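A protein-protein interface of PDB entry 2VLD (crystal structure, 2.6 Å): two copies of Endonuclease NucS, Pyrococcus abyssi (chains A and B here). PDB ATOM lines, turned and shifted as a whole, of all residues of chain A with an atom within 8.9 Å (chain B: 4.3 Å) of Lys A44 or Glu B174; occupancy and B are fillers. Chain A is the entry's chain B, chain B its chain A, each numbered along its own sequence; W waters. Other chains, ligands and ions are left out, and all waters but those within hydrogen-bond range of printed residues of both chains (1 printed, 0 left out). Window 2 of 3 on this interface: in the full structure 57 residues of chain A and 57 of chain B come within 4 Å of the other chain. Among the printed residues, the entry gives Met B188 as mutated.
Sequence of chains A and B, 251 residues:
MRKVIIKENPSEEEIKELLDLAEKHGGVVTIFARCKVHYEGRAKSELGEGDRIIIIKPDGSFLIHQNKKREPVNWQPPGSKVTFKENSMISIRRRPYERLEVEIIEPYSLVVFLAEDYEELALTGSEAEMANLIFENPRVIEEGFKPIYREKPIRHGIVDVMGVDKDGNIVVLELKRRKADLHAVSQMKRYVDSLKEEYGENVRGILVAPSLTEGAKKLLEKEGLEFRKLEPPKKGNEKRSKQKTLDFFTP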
ATOM      1  N   VAL A  37       4.398  20.108  18.850  1.00  0.00           N
ATOM      2  CA  VAL A  37       5.635  20.191  18.105  1.00  0.00           C
ATOM      3  C   VAL A  37       6.132  21.621  18.145  1.00  0.00           C
ATOM      4  O   VAL A  37       5.354  22.554  17.939  1.00  0.00           O
ATOM      5  CB  VAL A  37       5.446  19.732  16.633  1.00  0.00           C
ATOM      6  CG1 VAL A  37       6.756  19.813  15.860  1.00  0.00           C
ATOM      7  CG2 VAL A  37       4.889  18.314  16.569  1.00  0.00           C
ATOM      8  N   HIS A  38       7.422  21.773  18.426  1.00  0.00           N
ATOM      9  CA  HIS A  38       8.084  23.061  18.380  1.00  0.00           C
ATOM     10  C   HIS A  38       9.302  22.971  17.478  1.00  0.00           C
ATOM     11  O   HIS A  38      10.139  22.074  17.632  1.00  0.00           O
ATOM     12  CB  HIS A  38       8.525  23.489  19.772  1.00  0.00           C
ATOM     13  CG  HIS A  38       7.469  23.322  20.814  1.00  0.00           C
ATOM     14  ND1 HIS A  38       6.568  24.318  21.122  1.00  0.00           N
ATOM     15  CD2 HIS A  38       7.169  22.274  21.617  1.00  0.00           C
ATOM     16  CE1 HIS A  38       5.753  23.888  22.067  1.00  0.00           C
ATOM     17  NE2 HIS A  38       6.095  22.652  22.384  1.00  0.00           N
ATOM     18  N   TYR A  39       9.396  23.902  16.539  1.00  0.00           N
ATOM     19  CA  TYR A  39      10.485  23.924  15.586  1.00  0.00           C
ATOM     20  C   TYR A  39      11.204  25.251  15.686  1.00  0.00           C
ATOM     21  O   TYR A  39      10.572  26.304  15.808  1.00  0.00           O
ATOM     22  CB  TYR A  39       9.962  23.723  14.151  1.00  0.00           C
ATOM     23  CG  TYR A  39      11.059  23.821  13.109  1.00  0.00           C
ATOM     24  CD1 TYR A  39      11.956  22.773  12.926  1.00  0.00           C
ATOM     25  CD2 TYR A  39      11.217  24.970  12.327  1.00  0.00           C
ATOM     26  CE1 TYR A  39      12.983  22.854  11.997  1.00  0.00           C
ATOM     27  CE2 TYR A  39      12.245  25.063  11.376  1.00  0.00           C
ATOM     28  CZ  TYR A  39      13.128  23.990  11.228  1.00  0.00           C
ATOM     29  OH  TYR A  39      14.162  24.028  10.314  1.00  0.00           O
ATOM     30  N   GLU A  40      12.529  25.188  15.644  1.00  0.00           N
ATOM     31  CA  GLU A  40      13.364  26.365  15.479  1.00  0.00           C
ATOM     32  C   GLU A  40      14.422  26.047  14.437  1.00  0.00           C
ATOM     33  O   GLU A  40      15.277  25.190  14.656  1.00  0.00           O
ATOM     34  CB  GLU A  40      14.039  26.732  16.786  1.00  0.00           C
ATOM     35  CG  GLU A  40      13.107  27.272  17.833  1.00  0.00           C
ATOM     36  CD  GLU A  40      13.733  27.262  19.204  1.00  0.00           C
ATOM     37  OE1 GLU A  40      14.977  27.384  19.310  1.00  0.00           O
ATOM     38  OE2 GLU A  40      12.971  27.117  20.178  1.00  0.00           O
ATOM     39  N   GLY A  41      14.352  26.726  13.299  1.00  0.00           N
ATOM     40  CA  GLY A  41      15.332  26.539  12.232  1.00  0.00           C
ATOM     41  C   GLY A  41      15.623  27.890  11.628  1.00  0.00           C
ATOM     42  O   GLY A  41      16.180  28.760  12.294  1.00  0.00           O
ATOM     43  N   ARG A  42      15.233  28.085  10.374  1.00  0.00           N
ATOM     44  CA  ARG A  42      15.317  29.424   9.801  1.00  0.00           C
ATOM     45  C   ARG A  42      14.377  30.367  10.566  1.00  0.00           C
ATOM     46  O   ARG A  42      14.770  31.470  10.944  1.00  0.00           O
ATOM     47  CB  ARG A  42      15.015  29.422   8.301  1.00  0.00           C
ATOM     48  CG  ARG A  42      15.209  30.796   7.673  1.00  0.00           C
ATOM     49  CD  ARG A  42      15.132  30.785   6.153  1.00  0.00           C
ATOM     50  NE  ARG A  42      15.495  32.102   5.628  1.00  0.00           N
ATOM     51  CZ  ARG A  42      16.727  32.459   5.270  1.00  0.00           C
ATOM     52  NH1 ARG A  42      17.733  31.593   5.353  1.00  0.00           N
ATOM     53  NH2 ARG A  42      16.954  33.688   4.817  1.00  0.00           N
ATOM     54  N   ALA A  43      13.146  29.908  10.793  1.00  0.00           N
ATOM     55  CA  ALA A  43      12.166  30.612  11.619  1.00  0.00           C
ATOM     56  C   ALA A  43      11.642  29.702  12.730  1.00  0.00           C
ATOM     57  O   ALA A  43      12.159  28.603  12.944  1.00  0.00           O
ATOM     58  CB  ALA A  43      11.021  31.132  10.767  1.00  0.00           C
ATOM     59  N   LYS A  44      10.599  30.153  13.417  1.00  0.00           N
ATOM     60  CA  LYS A  44      10.168  29.540  14.656  1.00  0.00           C
ATOM     61  C   LYS A  44       8.689  29.277  14.604  1.00  0.00           C
ATOM     62  O   LYS A  44       7.889  30.191  14.441  1.00  0.00           O
ATOM     63  CB  LYS A  44      10.486  30.505  15.795  1.00  0.00           C
ATOM     64  CG  LYS A  44      10.416  29.965  17.207  1.00  0.00           C
ATOM     65  CD  LYS A  44      11.170  30.922  18.111  1.00  0.00           C
ATOM     66  CE  LYS A  44      10.621  30.941  19.517  1.00  0.00           C
ATOM     67  NZ  LYS A  44      11.265  32.000  20.334  1.00  0.00           N
ATOM     68  N   SER A  45       8.323  28.015  14.738  1.00  0.00           N
ATOM     69  CA  SER A  45       6.921  27.623  14.679  1.00  0.00           C
ATOM     70  C   SER A  45       6.585  26.587  15.741  1.00  0.00           C
ATOM     71  O   SER A  45       7.483  26.003  16.360  1.00  0.00           O
ATOM     72  CB  SER A  45       6.551  27.092  13.279  1.00  0.00           C
ATOM     73  OG  SER A  45       7.189  25.857  12.984  1.00  0.00           O
ATOM     74  N   GLU A  46       5.282  26.386  15.936  1.00  0.00           N
ATOM     75  CA  GLU A  46       4.736  25.298  16.756  1.00  0.00           C
ATOM     76  C   GLU A  46       3.460  24.693  16.152  1.00  0.00           C
ATOM     77  O   GLU A  46       2.794  25.312  15.324  1.00  0.00           O
ATOM     78  CB  GLU A  46       4.466  25.765  18.191  1.00  0.00           C
ATOM     79  CG  GLU A  46       3.520  26.937  18.329  1.00  0.00           C
ATOM     80  CD  GLU A  46       3.444  27.452  19.764  1.00  0.00           C
ATOM     81  OE1 GLU A  46       3.523  28.694  19.955  1.00  0.00           O
ATOM     82  OE2 GLU A  46       3.311  26.619  20.696  1.00  0.00           O
ATOM     83  N   LEU A  47       3.131  23.473  16.548  1.00  0.00           N
ATOM     84  CA  LEU A  47       1.828  22.926  16.221  1.00  0.00           C
ATOM     85  C   LEU A  47       1.209  22.510  17.537  1.00  0.00           C
ATOM     86  O   LEU A  47       1.907  21.988  18.406  1.00  0.00           O
ATOM     87  CB  LEU A  47       1.927  21.727  15.263  1.00  0.00           C
ATOM     88  CG  LEU A  47       2.649  21.818  13.914  1.00  0.00           C
ATOM     89  CD1 LEU A  47       2.568  20.471  13.227  1.00  0.00           C
ATOM     90  CD2 LEU A  47       2.108  22.911  13.000  1.00  0.00           C
ATOM     91  N   ASN A  74       6.939  17.684   9.943  1.00  0.00           N
ATOM     92  CA  ASN A  74       8.245  18.193  10.239  1.00  0.00           C
ATOM     93  C   ASN A  74       9.159  17.001  10.154  1.00  0.00           C
ATOM     94  O   ASN A  74       8.738  15.885  10.478  1.00  0.00           O
ATOM     95  CB  ASN A  74       8.263  18.746  11.658  1.00  0.00           C
ATOM     96  CG  ASN A  74       7.783  20.171  11.728  1.00  0.00           C
ATOM     97  OD1 ASN A  74       8.504  21.095  11.324  1.00  0.00           O
ATOM     98  ND2 ASN A  74       6.562  20.369  12.248  1.00  0.00           N
ATOM     99  N   ARG A  99      16.247  22.855  15.597  1.00  0.00           N
ATOM    100  CA  ARG A  99      15.727  22.111  16.735  1.00  0.00           C
ATOM    101  C   ARG A  99      14.287  21.704  16.488  1.00  0.00           C
ATOM    102  O   ARG A  99      13.415  22.548  16.274  1.00  0.00           O
ATOM    103  CB  ARG A  99      15.826  22.937  18.015  1.00  0.00           C
ATOM    104  CG  ARG A  99      15.952  22.099  19.276  1.00  0.00           C
ATOM    105  CD  ARG A  99      15.924  22.981  20.515  1.00  0.00           C
ATOM    106  NE  ARG A  99      14.594  23.019  21.103  1.00  0.00           N
ATOM    107  CZ  ARG A  99      14.271  22.418  22.240  1.00  0.00           C
ATOM    108  NH1 ARG A  99      15.184  21.745  22.926  1.00  0.00           N
ATOM    109  NH2 ARG A  99      13.034  22.499  22.699  1.00  0.00           N
ATOM    110  N   ILE B 158      16.180  30.908  18.685  1.00  0.00           N
ATOM    111  CA  ILE B 158      15.633  32.137  18.124  1.00  0.00           C
ATOM    112  C   ILE B 158      14.808  32.860  19.169  1.00  0.00           C
ATOM    113  O   ILE B 158      13.948  32.269  19.811  1.00  0.00           O
ATOM    114  CB  ILE B 158      14.814  31.845  16.894  1.00  0.00           C
ATOM    115  CG1 ILE B 158      15.653  30.988  15.936  1.00  0.00           C
ATOM    116  CG2 ILE B 158      14.335  33.148  16.251  1.00  0.00           C
ATOM    117  CD1 ILE B 158      15.139  30.933  14.517  1.00  0.00           C
ATOM    118  N   ASP B 160      12.316  35.881  20.452  1.00  0.00           N
ATOM    119  CA  ASP B 160      11.175  36.659  19.925  1.00  0.00           C
ATOM    120  C   ASP B 160      11.506  38.133  19.730  1.00  0.00           C
ATOM    121  O   ASP B 160      11.476  38.635  18.612  1.00  0.00           O
ATOM    122  CB  ASP B 160       9.941  36.491  20.828  1.00  0.00           C
ATOM    123  CG  ASP B 160       9.397  35.060  20.816  1.00  0.00           C
ATOM    124  OD1 ASP B 160       9.801  34.296  19.913  1.00  0.00           O
ATOM    125  OD2 ASP B 160       8.569  34.689  21.688  1.00  0.00           O
ATOM    126  N   VAL B 172      16.366  39.353  26.959  1.00  0.00           N
ATOM    127  CA  VAL B 172      15.624  38.427  26.118  1.00  0.00           C
ATOM    128  C   VAL B 172      14.135  38.487  26.458  1.00  0.00           C
ATOM    129  O   VAL B 172      13.772  38.364  27.622  1.00  0.00           O
ATOM    130  CB  VAL B 172      16.157  37.007  26.333  1.00  0.00           C
ATOM    131  CG1 VAL B 172      15.222  35.971  25.747  1.00  0.00           C
ATOM    132  CG2 VAL B 172      17.488  36.890  25.713  1.00  0.00           C
ATOM    133  N   LEU B 173      13.284  38.693  25.456  1.00  0.00           N
ATOM    134  CA  LEU B 173      11.823  38.559  25.627  1.00  0.00           C
ATOM    135  C   LEU B 173      11.289  37.325  24.901  1.00  0.00           C
ATOM    136  O   LEU B 173      11.569  37.112  23.721  1.00  0.00           O
ATOM    137  CB  LEU B 173      11.061  39.781  25.111  1.00  0.00           C
ATOM    138  CG  LEU B 173      11.310  41.200  25.610  1.00  0.00           C
ATOM    139  CD1 LEU B 173      10.274  42.134  24.985  1.00  0.00           C
ATOM    140  CD2 LEU B 173      11.267  41.284  27.124  1.00  0.00           C
ATOM    141  N   GLU B 174      10.529  36.511  25.622  1.00  0.00           N
ATOM    142  CA  GLU B 174       9.759  35.421  25.050  1.00  0.00           C
ATOM    143  C   GLU B 174       8.277  35.797  25.119  1.00  0.00           C
ATOM    144  O   GLU B 174       7.729  35.953  26.210  1.00  0.00           O
ATOM    145  CB  GLU B 174      10.032  34.135  25.832  1.00  0.00           C
ATOM    146  CG  GLU B 174       9.358  32.876  25.292  1.00  0.00           C
ATOM    147  CD  GLU B 174       9.933  32.404  23.960  1.00  0.00           C
ATOM    148  OE1 GLU B 174      10.873  33.043  23.430  1.00  0.00           O
ATOM    149  OE2 GLU B 174       9.435  31.389  23.430  1.00  0.00           O
ATOM    150  N   LEU B 175       7.643  35.961  23.959  1.00  0.00           N
ATOM    151  CA  LEU B 175       6.231  36.365  23.894  1.00  0.00           C
ATOM    152  C   LEU B 175       5.307  35.189  23.623  1.00  0.00           C
ATOM    153  O   LEU B 175       5.412  34.511  22.599  1.00  0.00           O
ATOM    154  CB  LEU B 175       5.987  37.426  22.812  1.00  0.00           C
ATOM    155  CG  LEU B 175       7.044  38.459  22.434  1.00  0.00           C
ATOM    156  CD1 LEU B 175       6.563  39.260  21.252  1.00  0.00           C
ATOM    157  CD2 LEU B 175       7.373  39.372  23.606  1.00  0.00           C
ATOM    158  N   LYS B 176       4.392  34.953  24.547  1.00  0.00           N
ATOM    159  CA  LYS B 176       3.294  34.024  24.314  1.00  0.00           C
ATOM    160  C   LYS B 176       1.997  34.825  24.366  1.00  0.00           C
ATOM    161  O   LYS B 176       1.943  35.876  25.005  1.00  0.00           O
ATOM    162  CB  LYS B 176       3.320  32.878  25.334  1.00  0.00           C
ATOM    163  CG  LYS B 176       4.544  31.952  25.184  1.00  0.00           C
ATOM    164  CD  LYS B 176       4.255  30.727  24.302  1.00  0.00           C
ATOM    165  CE  LYS B 176       5.392  30.443  23.294  1.00  0.00           C
ATOM    166  NZ  LYS B 176       6.715  30.017  23.868  1.00  0.00           N
ATOM    167  N   GLN B 187      11.849  27.141  27.454  1.00  0.00           N
ATOM    168  CA  GLN B 187      12.252  27.655  26.156  1.00  0.00           C
ATOM    169  C   GLN B 187      13.074  28.930  26.375  1.00  0.00           C
ATOM    170  O   GLN B 187      14.243  29.007  25.976  1.00  0.00           O
ATOM    171  CB  GLN B 187      11.031  27.859  25.238  1.00  0.00           C
ATOM    172  CG  GLN B 187      11.397  28.125  23.775  1.00  0.00           C
ATOM    173  CD  GLN B 187      10.284  27.816  22.746  1.00  0.00           C
ATOM    174  OE1 GLN B 187       9.875  26.660  22.584  1.00  0.00           O
ATOM    175  NE2 GLN B 187       9.840  28.845  22.015  1.00  0.00           N
ATOM    176  N   MET B 188      12.493  29.900  27.076  1.00  0.00           N
ATOM    177  CA  MET B 188      13.194  31.144  27.349  1.00  0.00           C
ATOM    178  C   MET B 188      14.512  30.926  28.100  1.00  0.00           C
ATOM    179  O   MET B 188      15.532  31.561  27.779  1.00  0.00           O
ATOM    180  CB  MET B 188      12.310  32.104  28.123  1.00  0.00           C
ATOM    181  CG  MET B 188      12.986  33.433  28.343  1.00  0.00           C
ATOM    182  SD  MET B 188      11.766  34.715  29.125  1.00  0.00           S
ATOM    183  CE  MET B 188      11.652  33.944  30.898  1.00  0.00           C
ATOM    184  N   TYR B 191      17.389  30.109  25.869  1.00  0.00           N
ATOM    185  CA  TYR B 191      17.874  31.299  25.174  1.00  0.00           C
ATOM    186  C   TYR B 191      18.758  32.108  26.089  1.00  0.00           C
ATOM    187  O   TYR B 191      19.841  32.524  25.693  1.00  0.00           O
ATOM    188  CB  TYR B 191      16.718  32.170  24.665  1.00  0.00           C
ATOM    189  CG  TYR B 191      15.716  31.450  23.796  1.00  0.00           C
ATOM    190  CD1 TYR B 191      14.363  31.768  23.865  1.00  0.00           C
ATOM    191  CD2 TYR B 191      16.115  30.451  22.903  1.00  0.00           C
ATOM    192  CE1 TYR B 191      13.435  31.122  23.075  1.00  0.00           C
ATOM    193  CE2 TYR B 191      15.192  29.788  22.104  1.00  0.00           C
ATOM    194  CZ  TYR B 191      13.853  30.129  22.195  1.00  0.00           C
ATOM    195  OH  TYR B 191      12.923  29.483  21.411  1.00  0.00           O
ATOM    196  N   ILE B 206      12.798  37.963  30.288  1.00  0.00           N
ATOM    197  CA  ILE B 206      11.440  38.367  30.636  1.00  0.00           C
ATOM    198  C   ILE B 206      10.413  37.637  29.773  1.00  0.00           C
ATOM    199  O   ILE B 206      10.422  37.752  28.545  1.00  0.00           O
ATOM    200  CB  ILE B 206      11.220  39.893  30.509  1.00  0.00           C
ATOM    201  CG1 ILE B 206      12.225  40.669  31.374  1.00  0.00           C
ATOM    202  CG2 ILE B 206       9.776  40.242  30.881  1.00  0.00           C
ATOM    203  CD1 ILE B 206      12.324  42.165  31.064  1.00  0.00           C
ATOM    204  N   LEU B 207       9.542  36.884  30.433  1.00  0.00           N
ATOM    205  CA  LEU B 207       8.447  36.193  29.778  1.00  0.00           C
ATOM    206  C   LEU B 207       7.259  37.137  29.641  1.00  0.00           C
ATOM    207  O   LEU B 207       6.693  37.554  30.642  1.00  0.00           O
ATOM    208  CB  LEU B 207       8.032  35.002  30.634  1.00  0.00           C
ATOM    209  CG  LEU B 207       7.427  33.731  30.044  1.00  0.00           C
ATOM    210  CD1 LEU B 207       6.554  33.144  31.129  1.00  0.00           C
ATOM    211  CD2 LEU B 207       6.620  33.962  28.781  1.00  0.00           C
ATOM    212  N   VAL B 208       6.879  37.465  28.409  1.00  0.00           N
ATOM    213  CA  VAL B 208       5.770  38.391  28.162  1.00  0.00           C
ATOM    214  C   VAL B 208       4.523  37.654  27.668  1.00  0.00           C
ATOM    215  O   VAL B 208       4.513  37.102  26.569  1.00  0.00           O
ATOM    216  CB  VAL B 208       6.153  39.507  27.157  1.00  0.00           C
ATOM    217  CG1 VAL B 208       5.011  40.491  26.987  1.00  0.00           C
ATOM    218  CG2 VAL B 208       7.410  40.229  27.603  1.00  0.00           C
HETATM  219  O   HOH W   1       6.935  26.919  20.815  1.00  0.00           O
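The side-chain carboxylate (OD1) of Asp B160 lies within salt-bridge range of the side-chain amino group (NZ) of Lys A44, 2.8 Å away. The backbone carbonyl oxygen of Ile B158 is in hydrogen-bond range of the side-chain amino group of Lys A44, 2.7 Å away. The side-chain hydroxyl (OH) of Tyr B191 is in hydrogen-bond range of the side-chain carboxylate (OE2) of Glu A40, 2.7 Å away. OE1 of Glu B174 lies within salt-bridge range of NZ of Lys A44, at 3.3 Å. OH of Tyr B191 sits at hydrogen-bond distance from NZ of Lys A44 (3.2 Å).
Of the 13 printed residues of chain B, 5 touch a printed residue of chain A. Hydrophobic or aromatic side chains of chain B within 4 Å of the printed part of chain A: Ile B158 and Tyr B191. Among the printed residues, 10 pairs touch across the chains.
The backbone carbonyl oxygen of Ile B158 lies close to the side-chain hydroxyl of Tyr B191, 3.4 Å away. The backbone NH of Glu B174 sits at hydrogen-bond distance from the backbone carbonyl oxygen of Ile B206 (3.2 Å). The side-chain carboxylate of Glu B174 sits at hydrogen-bond distance from the side-chain amide nitrogen of Gln B187, at 2.9 Å. The backbone NH (N) of Leu B175 sits at hydrogen-bond distance from the side-chain carboxylate (OD2) of Asp B160 (2.8 Å). O of Glu A40 lies within hydrogen-bond range of N of Arg A99 (2.7 Å). N of Val B208 is in hydrogen-bond range of O of Glu B174, 2.8 Å away.
Lys A44 touches five residues of chain B. Glu B174 touches just one residue of chain A: Lys A44. Printed residues of chain B within 4 Å of Glu A40: Ile B158, Gln B187 and Tyr B191. Printed residues of chain A within 4 Å of Ile B158: Glu A40, Gly A41, Arg A42 and Lys A44. Of the printed residues of chain B, Gly A41 touches Ile B158 (3.3 Å). The nearest printed residue of chain B that does not touch Lys A44 is Lys B176 (5.9 Å). The nearest residue of chain A that does not touch Glu B174 is Glu A40 (6.4 Å). The nearest printed residue of chain B that does not touch Glu A40 is Glu B174 (6.4 Å).
Water W1 lies within hydrogen-bond range of a ring nitrogen (ND1) of His A38 and the side-chain amide oxygen (OE1) of Gln B187.
Among the printed residues, merely in contact across the chains: Glu A40 with Ile B158 (3.8 Å), Glu A40 with Gln B187 (3.8 Å), Gly A41 with Ile B158 (3.3 Å), Arg A42 with Ile B158 (3.6 Å) and Lys A44 with Gln B187 (3.4 Å).
No position is printed for both chains. Of the 10 pairs that touch across the chains among the printed residues, none has its exchanged pair printed and touching as well.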
